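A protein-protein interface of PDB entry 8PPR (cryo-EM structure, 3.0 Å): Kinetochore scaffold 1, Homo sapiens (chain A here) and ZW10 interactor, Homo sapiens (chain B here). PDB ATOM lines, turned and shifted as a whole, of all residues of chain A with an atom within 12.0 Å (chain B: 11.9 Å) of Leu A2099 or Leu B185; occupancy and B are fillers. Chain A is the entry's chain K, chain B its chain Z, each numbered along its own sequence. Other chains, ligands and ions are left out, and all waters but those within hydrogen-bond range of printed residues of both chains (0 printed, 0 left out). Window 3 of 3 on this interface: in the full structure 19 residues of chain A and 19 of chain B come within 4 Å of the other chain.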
ATOM      1  N   ARG A2097      -4.262  10.750  10.060  1.00  0.00           N
ATOM      2  CA  ARG A2097      -3.247  11.434   9.268  1.00  0.00           C
ATOM      3  C   ARG A2097      -2.028  11.767  10.122  1.00  0.00           C
ATOM      4  O   ARG A2097      -0.886  11.588   9.692  1.00  0.00           O
ATOM      5  CB  ARG A2097      -3.823  12.706   8.642  1.00  0.00           C
ATOM      6  CG  ARG A2097      -2.973  13.289   7.526  1.00  0.00           C
ATOM      7  CD  ARG A2097      -3.581  14.573   6.985  1.00  0.00           C
ATOM      8  NE  ARG A2097      -4.861  14.334   6.331  1.00  0.00           N
ATOM      9  CZ  ARG A2097      -5.662  15.290   5.881  1.00  0.00           C
ATOM     10  NH1 ARG A2097      -5.345  16.570   5.996  1.00  0.00           N
ATOM     11  NH2 ARG A2097      -6.811  14.954   5.300  1.00  0.00           N
ATOM     12  N   ASN A2098      -2.279  12.257  11.339  1.00  0.00           N
ATOM     13  CA  ASN A2098      -1.186  12.551  12.259  1.00  0.00           C
ATOM     14  C   ASN A2098      -0.424  11.284  12.628  1.00  0.00           C
ATOM     15  O   ASN A2098       0.810  11.293  12.714  1.00  0.00           O
ATOM     16  CB  ASN A2098      -1.726  13.238  13.514  1.00  0.00           C
ATOM     17  CG  ASN A2098      -2.187  14.657  13.248  1.00  0.00           C
ATOM     18  OD1 ASN A2098      -1.824  15.261  12.239  1.00  0.00           O
ATOM     19  ND2 ASN A2098      -2.993  15.197  14.155  1.00  0.00           N
ATOM     20  N   LEU A2099      -1.146  10.183  12.855  1.00  0.00           N
ATOM     21  CA  LEU A2099      -0.491   8.914  13.157  1.00  0.00           C
ATOM     22  C   LEU A2099       0.369   8.448  11.990  1.00  0.00           C
ATOM     23  O   LEU A2099       1.490   7.966  12.189  1.00  0.00           O
ATOM     24  CB  LEU A2099      -1.537   7.858  13.511  1.00  0.00           C
ATOM     25  CG  LEU A2099      -1.007   6.496  13.963  1.00  0.00           C
ATOM     26  CD1 LEU A2099      -0.357   6.603  15.332  1.00  0.00           C
ATOM     27  CD2 LEU A2099      -2.124   5.464  13.974  1.00  0.00           C
ATOM     28  N   LEU A2100      -0.140   8.580  10.763  1.00  0.00           N
ATOM     29  CA  LEU A2100       0.638   8.196   9.590  1.00  0.00           C
ATOM     30  C   LEU A2100       1.887   9.058   9.448  1.00  0.00           C
ATOM     31  O   LEU A2100       2.969   8.550   9.128  1.00  0.00           O
ATOM     32  CB  LEU A2100      -0.227   8.293   8.334  1.00  0.00           C
ATOM     33  CG  LEU A2100      -1.302   7.217   8.169  1.00  0.00           C
ATOM     34  CD1 LEU A2100      -2.204   7.534   6.986  1.00  0.00           C
ATOM     35  CD2 LEU A2100      -0.671   5.842   8.013  1.00  0.00           C
ATOM     36  N   GLU A2101       1.755  10.367   9.676  1.00  0.00           N
ATOM     37  CA  GLU A2101       2.913  11.253   9.595  1.00  0.00           C
ATOM     38  C   GLU A2101       3.952  10.900  10.653  1.00  0.00           C
ATOM     39  O   GLU A2101       5.158  10.893  10.374  1.00  0.00           O
ATOM     40  CB  GLU A2101       2.470  12.707   9.741  1.00  0.00           C
ATOM     41  CG  GLU A2101       3.581  13.721   9.526  1.00  0.00           C
ATOM     42  CD  GLU A2101       3.077  15.151   9.555  1.00  0.00           C
ATOM     43  OE1 GLU A2101       1.884  15.356   9.861  1.00  0.00           O
ATOM     44  OE2 GLU A2101       3.875  16.070   9.273  1.00  0.00           O
ATOM     45  N   LEU A2102       3.504  10.599  11.874  1.00  0.00           N
ATOM     46  CA  LEU A2102       4.435  10.212  12.928  1.00  0.00           C
ATOM     47  C   LEU A2102       5.115   8.888  12.604  1.00  0.00           C
ATOM     48  O   LEU A2102       6.306   8.712  12.885  1.00  0.00           O
ATOM     49  CB  LEU A2102       3.709  10.134  14.270  1.00  0.00           C
ATOM     50  CG  LEU A2102       3.453  11.464  14.983  1.00  0.00           C
ATOM     51  CD1 LEU A2102       2.958  11.225  16.400  1.00  0.00           C
ATOM     52  CD2 LEU A2102       4.708  12.323  14.988  1.00  0.00           C
ATOM     53  N   GLU A2103       4.379   7.944  12.012  1.00  0.00           N
ATOM     54  CA  GLU A2103       4.984   6.680  11.605  1.00  0.00           C
ATOM     55  C   GLU A2103       6.031   6.894  10.517  1.00  0.00           C
ATOM     56  O   GLU A2103       7.094   6.261  10.533  1.00  0.00           O
ATOM     57  CB  GLU A2103       3.901   5.712  11.127  1.00  0.00           C
ATOM     58  CG  GLU A2103       3.241   4.920  12.243  1.00  0.00           C
ATOM     59  CD  GLU A2103       2.107   4.046  11.744  1.00  0.00           C
ATOM     60  OE1 GLU A2103       1.819   4.079  10.530  1.00  0.00           O
ATOM     61  OE2 GLU A2103       1.504   3.326  12.568  1.00  0.00           O
ATOM     62  N   VAL A2104       5.744   7.779   9.560  1.00  0.00           N
ATOM     63  CA  VAL A2104       6.716   8.088   8.513  1.00  0.00           C
ATOM     64  C   VAL A2104       7.963   8.724   9.115  1.00  0.00           C
ATOM     65  O   VAL A2104       9.095   8.396   8.734  1.00  0.00           O
ATOM     66  CB  VAL A2104       6.076   8.991   7.441  1.00  0.00           C
ATOM     67  CG1 VAL A2104       7.141   9.575   6.524  1.00  0.00           C
ATOM     68  CG2 VAL A2104       5.048   8.211   6.637  1.00  0.00           C
ATOM     69  N   GLN A2105       7.776   9.646  10.063  1.00  0.00           N
ATOM     70  CA  GLN A2105       8.915  10.269  10.731  1.00  0.00           C
ATOM     71  C   GLN A2105       9.736   9.238  11.497  1.00  0.00           C
ATOM     72  O   GLN A2105      10.971   9.286  11.492  1.00  0.00           O
ATOM     73  CB  GLN A2105       8.430  11.374  11.668  1.00  0.00           C
ATOM     74  CG  GLN A2105       7.996  12.644  10.955  1.00  0.00           C
ATOM     75  CD  GLN A2105       7.540  13.723  11.917  1.00  0.00           C
ATOM     76  OE1 GLN A2105       7.759  13.628  13.124  1.00  0.00           O
ATOM     77  NE2 GLN A2105       6.899  14.758  11.385  1.00  0.00           N
ATOM     78  N   LYS A2106       9.062   8.300  12.168  1.00  0.00           N
ATOM     79  CA  LYS A2106       9.763   7.240  12.885  1.00  0.00           C
ATOM     80  C   LYS A2106      10.560   6.358  11.931  1.00  0.00           C
ATOM     81  O   LYS A2106      11.697   5.975  12.230  1.00  0.00           O
ATOM     82  CB  LYS A2106       8.758   6.405  13.680  1.00  0.00           C
ATOM     83  CG  LYS A2106       9.340   5.159  14.317  1.00  0.00           C
ATOM     84  CD  LYS A2106       8.248   4.293  14.920  1.00  0.00           C
ATOM     85  CE  LYS A2106       8.782   2.931  15.328  1.00  0.00           C
ATOM     86  NZ  LYS A2106       7.708   2.058  15.877  1.00  0.00           N
ATOM     87  N   GLU A2107       9.975   6.019  10.780  1.00  0.00           N
ATOM     88  CA  GLU A2107      10.692   5.220   9.790  1.00  0.00           C
ATOM     89  C   GLU A2107      11.913   5.964   9.263  1.00  0.00           C
ATOM     90  O   GLU A2107      12.983   5.369   9.081  1.00  0.00           O
ATOM     91  CB  GLU A2107       9.757   4.840   8.643  1.00  0.00           C
ATOM     92  CG  GLU A2107      10.330   3.799   7.694  1.00  0.00           C
ATOM     93  CD  GLU A2107      10.525   2.449   8.356  1.00  0.00           C
ATOM     94  OE1 GLU A2107       9.744   2.116   9.273  1.00  0.00           O
ATOM     95  OE2 GLU A2107      11.458   1.720   7.960  1.00  0.00           O
ATOM     96  N   GLN A2108      11.772   7.266   9.009  1.00  0.00           N
ATOM     97  CA  GLN A2108      12.911   8.061   8.558  1.00  0.00           C
ATOM     98  C   GLN A2108      14.003   8.111   9.621  1.00  0.00           C
ATOM     99  O   GLN A2108      15.196   8.017   9.304  1.00  0.00           O
ATOM    100  CB  GLN A2108      12.452   9.471   8.189  1.00  0.00           C
ATOM    101  CG  GLN A2108      11.691   9.550   6.875  1.00  0.00           C
ATOM    102  CD  GLN A2108      11.183  10.947   6.579  1.00  0.00           C
ATOM    103  OE1 GLN A2108      11.199  11.823   7.445  1.00  0.00           O
ATOM    104  NE2 GLN A2108      10.728  11.163   5.350  1.00  0.00           N
ATOM    105  N   THR A2109      13.613   8.261  10.889  1.00  0.00           N
ATOM    106  CA  THR A2109      14.590   8.264  11.972  1.00  0.00           C
ATOM    107  C   THR A2109      15.314   6.926  12.063  1.00  0.00           C
ATOM    108  O   THR A2109      16.532   6.884  12.266  1.00  0.00           O
ATOM    109  CB  THR A2109      13.905   8.595  13.299  1.00  0.00           C
ATOM    110  OG1 THR A2109      13.144   9.800  13.158  1.00  0.00           O
ATOM    111  CG2 THR A2109      14.937   8.779  14.402  1.00  0.00           C
ATOM    112  N   GLN B 183      -4.287   7.251  22.023  1.00  0.00           N
ATOM    113  CA  GLN B 183      -3.362   6.378  22.737  1.00  0.00           C
ATOM    114  C   GLN B 183      -2.262   5.878  21.808  1.00  0.00           C
ATOM    115  O   GLN B 183      -1.080   5.915  22.152  1.00  0.00           O
ATOM    116  CB  GLN B 183      -4.111   5.198  23.358  1.00  0.00           C
ATOM    117  CG  GLN B 183      -5.010   5.582  24.521  1.00  0.00           C
ATOM    118  CD  GLN B 183      -5.823   4.414  25.041  1.00  0.00           C
ATOM    119  OE1 GLN B 183      -5.855   3.345  24.431  1.00  0.00           O
ATOM    120  NE2 GLN B 183      -6.485   4.611  26.174  1.00  0.00           N
ATOM    121  N   GLU B 184      -2.664   5.404  20.626  1.00  0.00           N
ATOM    122  CA  GLU B 184      -1.687   4.964  19.636  1.00  0.00           C
ATOM    123  C   GLU B 184      -0.804   6.120  19.186  1.00  0.00           C
ATOM    124  O   GLU B 184       0.410   5.956  19.014  1.00  0.00           O
ATOM    125  CB  GLU B 184      -2.399   4.334  18.438  1.00  0.00           C
ATOM    126  CG  GLU B 184      -1.466   3.663  17.441  1.00  0.00           C
ATOM    127  CD  GLU B 184      -0.876   2.370  17.971  1.00  0.00           C
ATOM    128  OE1 GLU B 184      -1.482   1.766  18.882  1.00  0.00           O
ATOM    129  OE2 GLU B 184       0.194   1.957  17.475  1.00  0.00           O
ATOM    130  N   LEU B 185      -1.399   7.301  18.991  1.00  0.00           N
ATOM    131  CA  LEU B 185      -0.615   8.473  18.616  1.00  0.00           C
ATOM    132  C   LEU B 185       0.389   8.833  19.703  1.00  0.00           C
ATOM    133  O   LEU B 185       1.545   9.154  19.408  1.00  0.00           O
ATOM    134  CB  LEU B 185      -1.544   9.652  18.329  1.00  0.00           C
ATOM    135  CG  LEU B 185      -0.891  10.935  17.810  1.00  0.00           C
ATOM    136  CD1 LEU B 185      -0.723  10.877  16.300  1.00  0.00           C
ATOM    137  CD2 LEU B 185      -1.706  12.154  18.215  1.00  0.00           C
ATOM    138  N   ASP B 186      -0.034   8.782  20.970  1.00  0.00           N
ATOM    139  CA  ASP B 186       0.877   9.079  22.071  1.00  0.00           C
ATOM    140  C   ASP B 186       2.011   8.062  22.142  1.00  0.00           C
ATOM    141  O   ASP B 186       3.171   8.427  22.370  1.00  0.00           O
ATOM    142  CB  ASP B 186       0.106   9.118  23.390  1.00  0.00           C
ATOM    143  CG  ASP B 186      -0.792  10.333  23.505  1.00  0.00           C
ATOM    144  OD1 ASP B 186      -0.592  11.296  22.735  1.00  0.00           O
ATOM    145  OD2 ASP B 186      -1.699  10.325  24.364  1.00  0.00           O
ATOM    146  N   ARG B 187       1.692   6.777  21.957  1.00  0.00           N
ATOM    147  CA  ARG B 187       2.726   5.748  21.979  1.00  0.00           C
ATOM    148  C   ARG B 187       3.724   5.943  20.844  1.00  0.00           C
ATOM    149  O   ARG B 187       4.938   5.808  21.043  1.00  0.00           O
ATOM    150  CB  ARG B 187       2.083   4.362  21.896  1.00  0.00           C
ATOM    151  CG  ARG B 187       3.014   3.219  22.261  1.00  0.00           C
ATOM    152  CD  ARG B 187       2.309   1.878  22.130  1.00  0.00           C
ATOM    153  NE  ARG B 187       3.190   0.761  22.448  1.00  0.00           N
ATOM    154  CZ  ARG B 187       2.813  -0.510  22.457  1.00  0.00           C
ATOM    155  NH1 ARG B 187       1.572  -0.865  22.169  1.00  0.00           N
ATOM    156  NH2 ARG B 187       3.703  -1.448  22.765  1.00  0.00           N
ATOM    157  N   VAL B 188       3.232   6.266  19.647  1.00  0.00           N
ATOM    158  CA  VAL B 188       4.124   6.485  18.514  1.00  0.00           C
ATOM    159  C   VAL B 188       4.980   7.726  18.742  1.00  0.00           C
ATOM    160  O   VAL B 188       6.163   7.752  18.383  1.00  0.00           O
ATOM    161  CB  VAL B 188       3.313   6.576  17.207  1.00  0.00           C
ATOM    162  CG1 VAL B 188       4.186   7.073  16.066  1.00  0.00           C
ATOM    163  CG2 VAL B 188       2.714   5.221  16.865  1.00  0.00           C
ATOM    164  N   PHE B 189       4.406   8.766  19.351  1.00  0.00           N
ATOM    165  CA  PHE B 189       5.184   9.961  19.668  1.00  0.00           C
ATOM    166  C   PHE B 189       6.285   9.653  20.677  1.00  0.00           C
ATOM    167  O   PHE B 189       7.414  10.138  20.542  1.00  0.00           O
ATOM    168  CB  PHE B 189       4.261  11.058  20.198  1.00  0.00           C
ATOM    169  CG  PHE B 189       4.906  12.413  20.263  1.00  0.00           C
ATOM    170  CD1 PHE B 189       4.999  13.207  19.133  1.00  0.00           C
ATOM    171  CD2 PHE B 189       5.416  12.895  21.459  1.00  0.00           C
ATOM    172  CE1 PHE B 189       5.591  14.454  19.192  1.00  0.00           C
ATOM    173  CE2 PHE B 189       6.008  14.140  21.524  1.00  0.00           C
ATOM    174  CZ  PHE B 189       6.096  14.921  20.389  1.00  0.00           C
ATOM    175  N   GLN B 190       5.972   8.852  21.698  1.00  0.00           N
ATOM    176  CA  GLN B 190       6.989   8.465  22.673  1.00  0.00           C
ATOM    177  C   GLN B 190       8.094   7.642  22.020  1.00  0.00           C
ATOM    178  O   GLN B 190       9.282   7.838  22.308  1.00  0.00           O
ATOM    179  CB  GLN B 190       6.345   7.688  23.821  1.00  0.00           C
ATOM    180  CG  GLN B 190       5.586   8.555  24.810  1.00  0.00           C
ATOM    181  CD  GLN B 190       4.968   7.751  25.936  1.00  0.00           C
ATOM    182  OE1 GLN B 190       5.227   6.555  26.074  1.00  0.00           O
ATOM    183  NE2 GLN B 190       4.145   8.403  26.748  1.00  0.00           N
ATOM    184  N   LYS B 191       7.718   6.711  21.139  1.00  0.00           N
ATOM    185  CA  LYS B 191       8.716   5.917  20.430  1.00  0.00           C
ATOM    186  C   LYS B 191       9.593   6.796  19.546  1.00  0.00           C
ATOM    187  O   LYS B 191      10.812   6.597  19.472  1.00  0.00           O
ATOM    188  CB  LYS B 191       8.028   4.834  19.599  1.00  0.00           C
ATOM    189  CG  LYS B 191       7.535   3.649  20.413  1.00  0.00           C
ATOM    190  CD  LYS B 191       6.895   2.595  19.525  1.00  0.00           C
ATOM    191  CE  LYS B 191       6.352   1.438  20.349  1.00  0.00           C
ATOM    192  NZ  LYS B 191       5.630   0.446  19.506  1.00  0.00           N
ATOM    193  N   LEU B 192       8.988   7.774  18.868  1.00  0.00           N
ATOM    194  CA  LEU B 192       9.754   8.693  18.036  1.00  0.00           C
ATOM    195  C   LEU B 192      10.712   9.527  18.874  1.00  0.00           C
ATOM    196  O   LEU B 192      11.852   9.773  18.465  1.00  0.00           O
ATOM    197  CB  LEU B 192       8.807   9.593  17.242  1.00  0.00           C
ATOM    198  CG  LEU B 192       9.452  10.682  16.382  1.00  0.00           C
ATOM    199  CD1 LEU B 192      10.366  10.066  15.334  1.00  0.00           C
ATOM    200  CD2 LEU B 192       8.388  11.549  15.728  1.00  0.00           C
ATOM    201  N   GLY B 193      10.267   9.978  20.048  1.00  0.00           N
ATOM    202  CA  GLY B 193      11.158  10.716  20.931  1.00  0.00           C
ATOM    203  C   GLY B 193      12.326   9.877  21.415  1.00  0.00           C
ATOM    204  O   GLY B 193      13.465  10.350  21.469  1.00  0.00           O
ATOM    205  N   ASN B 194      12.060   8.620  21.777  1.00  0.00           N
ATOM    206  CA  ASN B 194      13.139   7.728  22.194  1.00  0.00           C
ATOM    207  C   ASN B 194      14.121   7.483  21.054  1.00  0.00           C
ATOM    208  O   ASN B 194      15.342   7.471  21.264  1.00  0.00           O
ATOM    209  CB  ASN B 194      12.562   6.407  22.700  1.00  0.00           C
ATOM    210  CG  ASN B 194      11.783   6.569  23.990  1.00  0.00           C
ATOM    211  OD1 ASN B 194      11.935   7.563  24.699  1.00  0.00           O
ATOM    212  ND2 ASN B 194      10.942   5.589  24.299  1.00  0.00           N
ATOM    213  N   LYS B 196      14.697   9.525  18.573  1.00  0.00           N
ATOM    214  CA  LYS B 196      15.433  10.772  18.389  1.00  0.00           C
ATOM    215  C   LYS B 196      16.541  10.918  19.425  1.00  0.00           C
ATOM    216  O   LYS B 196      17.636  11.392  19.107  1.00  0.00           O
ATOM    217  CB  LYS B 196      14.472  11.958  18.456  1.00  0.00           C
ATOM    218  CG  LYS B 196      13.732  12.229  17.158  1.00  0.00           C
ATOM    219  CD  LYS B 196      12.871  13.476  17.263  1.00  0.00           C
ATOM    220  CE  LYS B 196      12.190  13.789  15.941  1.00  0.00           C
ATOM    221  NZ  LYS B 196      11.276  14.960  16.051  1.00  0.00           N
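The backbone carbonyl oxygen of Gln A2105 is in hydrogen-bond range of the side-chain hydroxyl of Thr A2109, 2.8 Å away.
Among the printed residues, merely in contact across the chains: Gln A2105 with Leu B192 (3.4 Å), Thr A2109 with Leu B192 (3.5 Å), Leu A2099 with Leu B185 (3.5 Å), Leu A2102 with Val B188 (3.6 Å), Leu A2102 with Leu B185 (3.7 Å), Leu A2099 with Val B188 (3.7 Å), Asn A2098 with Leu B185 (3.7 Å), Lys A2106 with Lys B191 (3.8 Å), Leu A2099 with Glu B184 (3.8 Å), Lys A2106 with Leu B192 (3.8 Å), Leu A2102 with Leu B192 (3.8 Å) and Leu A2102 with Phe B189 (3.9 Å).
Of chain B, only Glu B184 (3.8 Å), Leu B185 (3.5 Å) and Val B188 (3.7 Å) come within 4 Å of Leu A2099. No residue of chain B comes within 4 Å of Leu A2100. Leu A2102 touches just these residues of chain B: Leu B185, Val B188, Phe B189 and Leu B192. No residue of chain B comes within 4 Å of Glu A2103. Of the printed residues of chain B, Gln A2105 touches Leu B192. Of the printed residues of chain B, Lys A2106 touches Lys B191 (3.8 Å) and Leu B192 (3.8 Å). Glu B184 touches just one residue of chain A: Leu A2099 (3.8 Å). Leu B185 touches just these residues of chain A: Asn A2098 (3.7 Å), Leu A2099 (3.5 Å) and Leu A2102 (3.7 Å). No residue of chain A comes within 4 Å of Asp B186. Of chain A, only Leu A2102 (3.9 Å) comes within 4 Å of Phe B189. Printed residues of chain A within 4 Å of Leu B192: Leu A2102, Gln A2105, Lys A2106 and Thr A2109. The nearest residue of chain A that does not touch Leu B185 is Leu A2100 (6.0 Å).
Printed residues of chain A that touch a printed residue of chain B: Asn A2098, Leu A2099, Leu A2102, Gln A2105, Lys A2106 and Thr A2109. Printed residues of chain B that touch a printed residue of chain A: Glu B184, Leu B185, Val B188, Phe B189, Lys B191 and Leu B192. Hydrophobic or aromatic side chains of chain B within 4 Å of the printed part of chain A: Leu B185, Val B188, Phe B189 and Leu B192. Among the printed residues, 12 pairs touch across the chains. Among the printed residues, no Asp or Glu carboxylate lies within 4 Å of a Lys or Arg side-chain nitrogen of the other chain.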
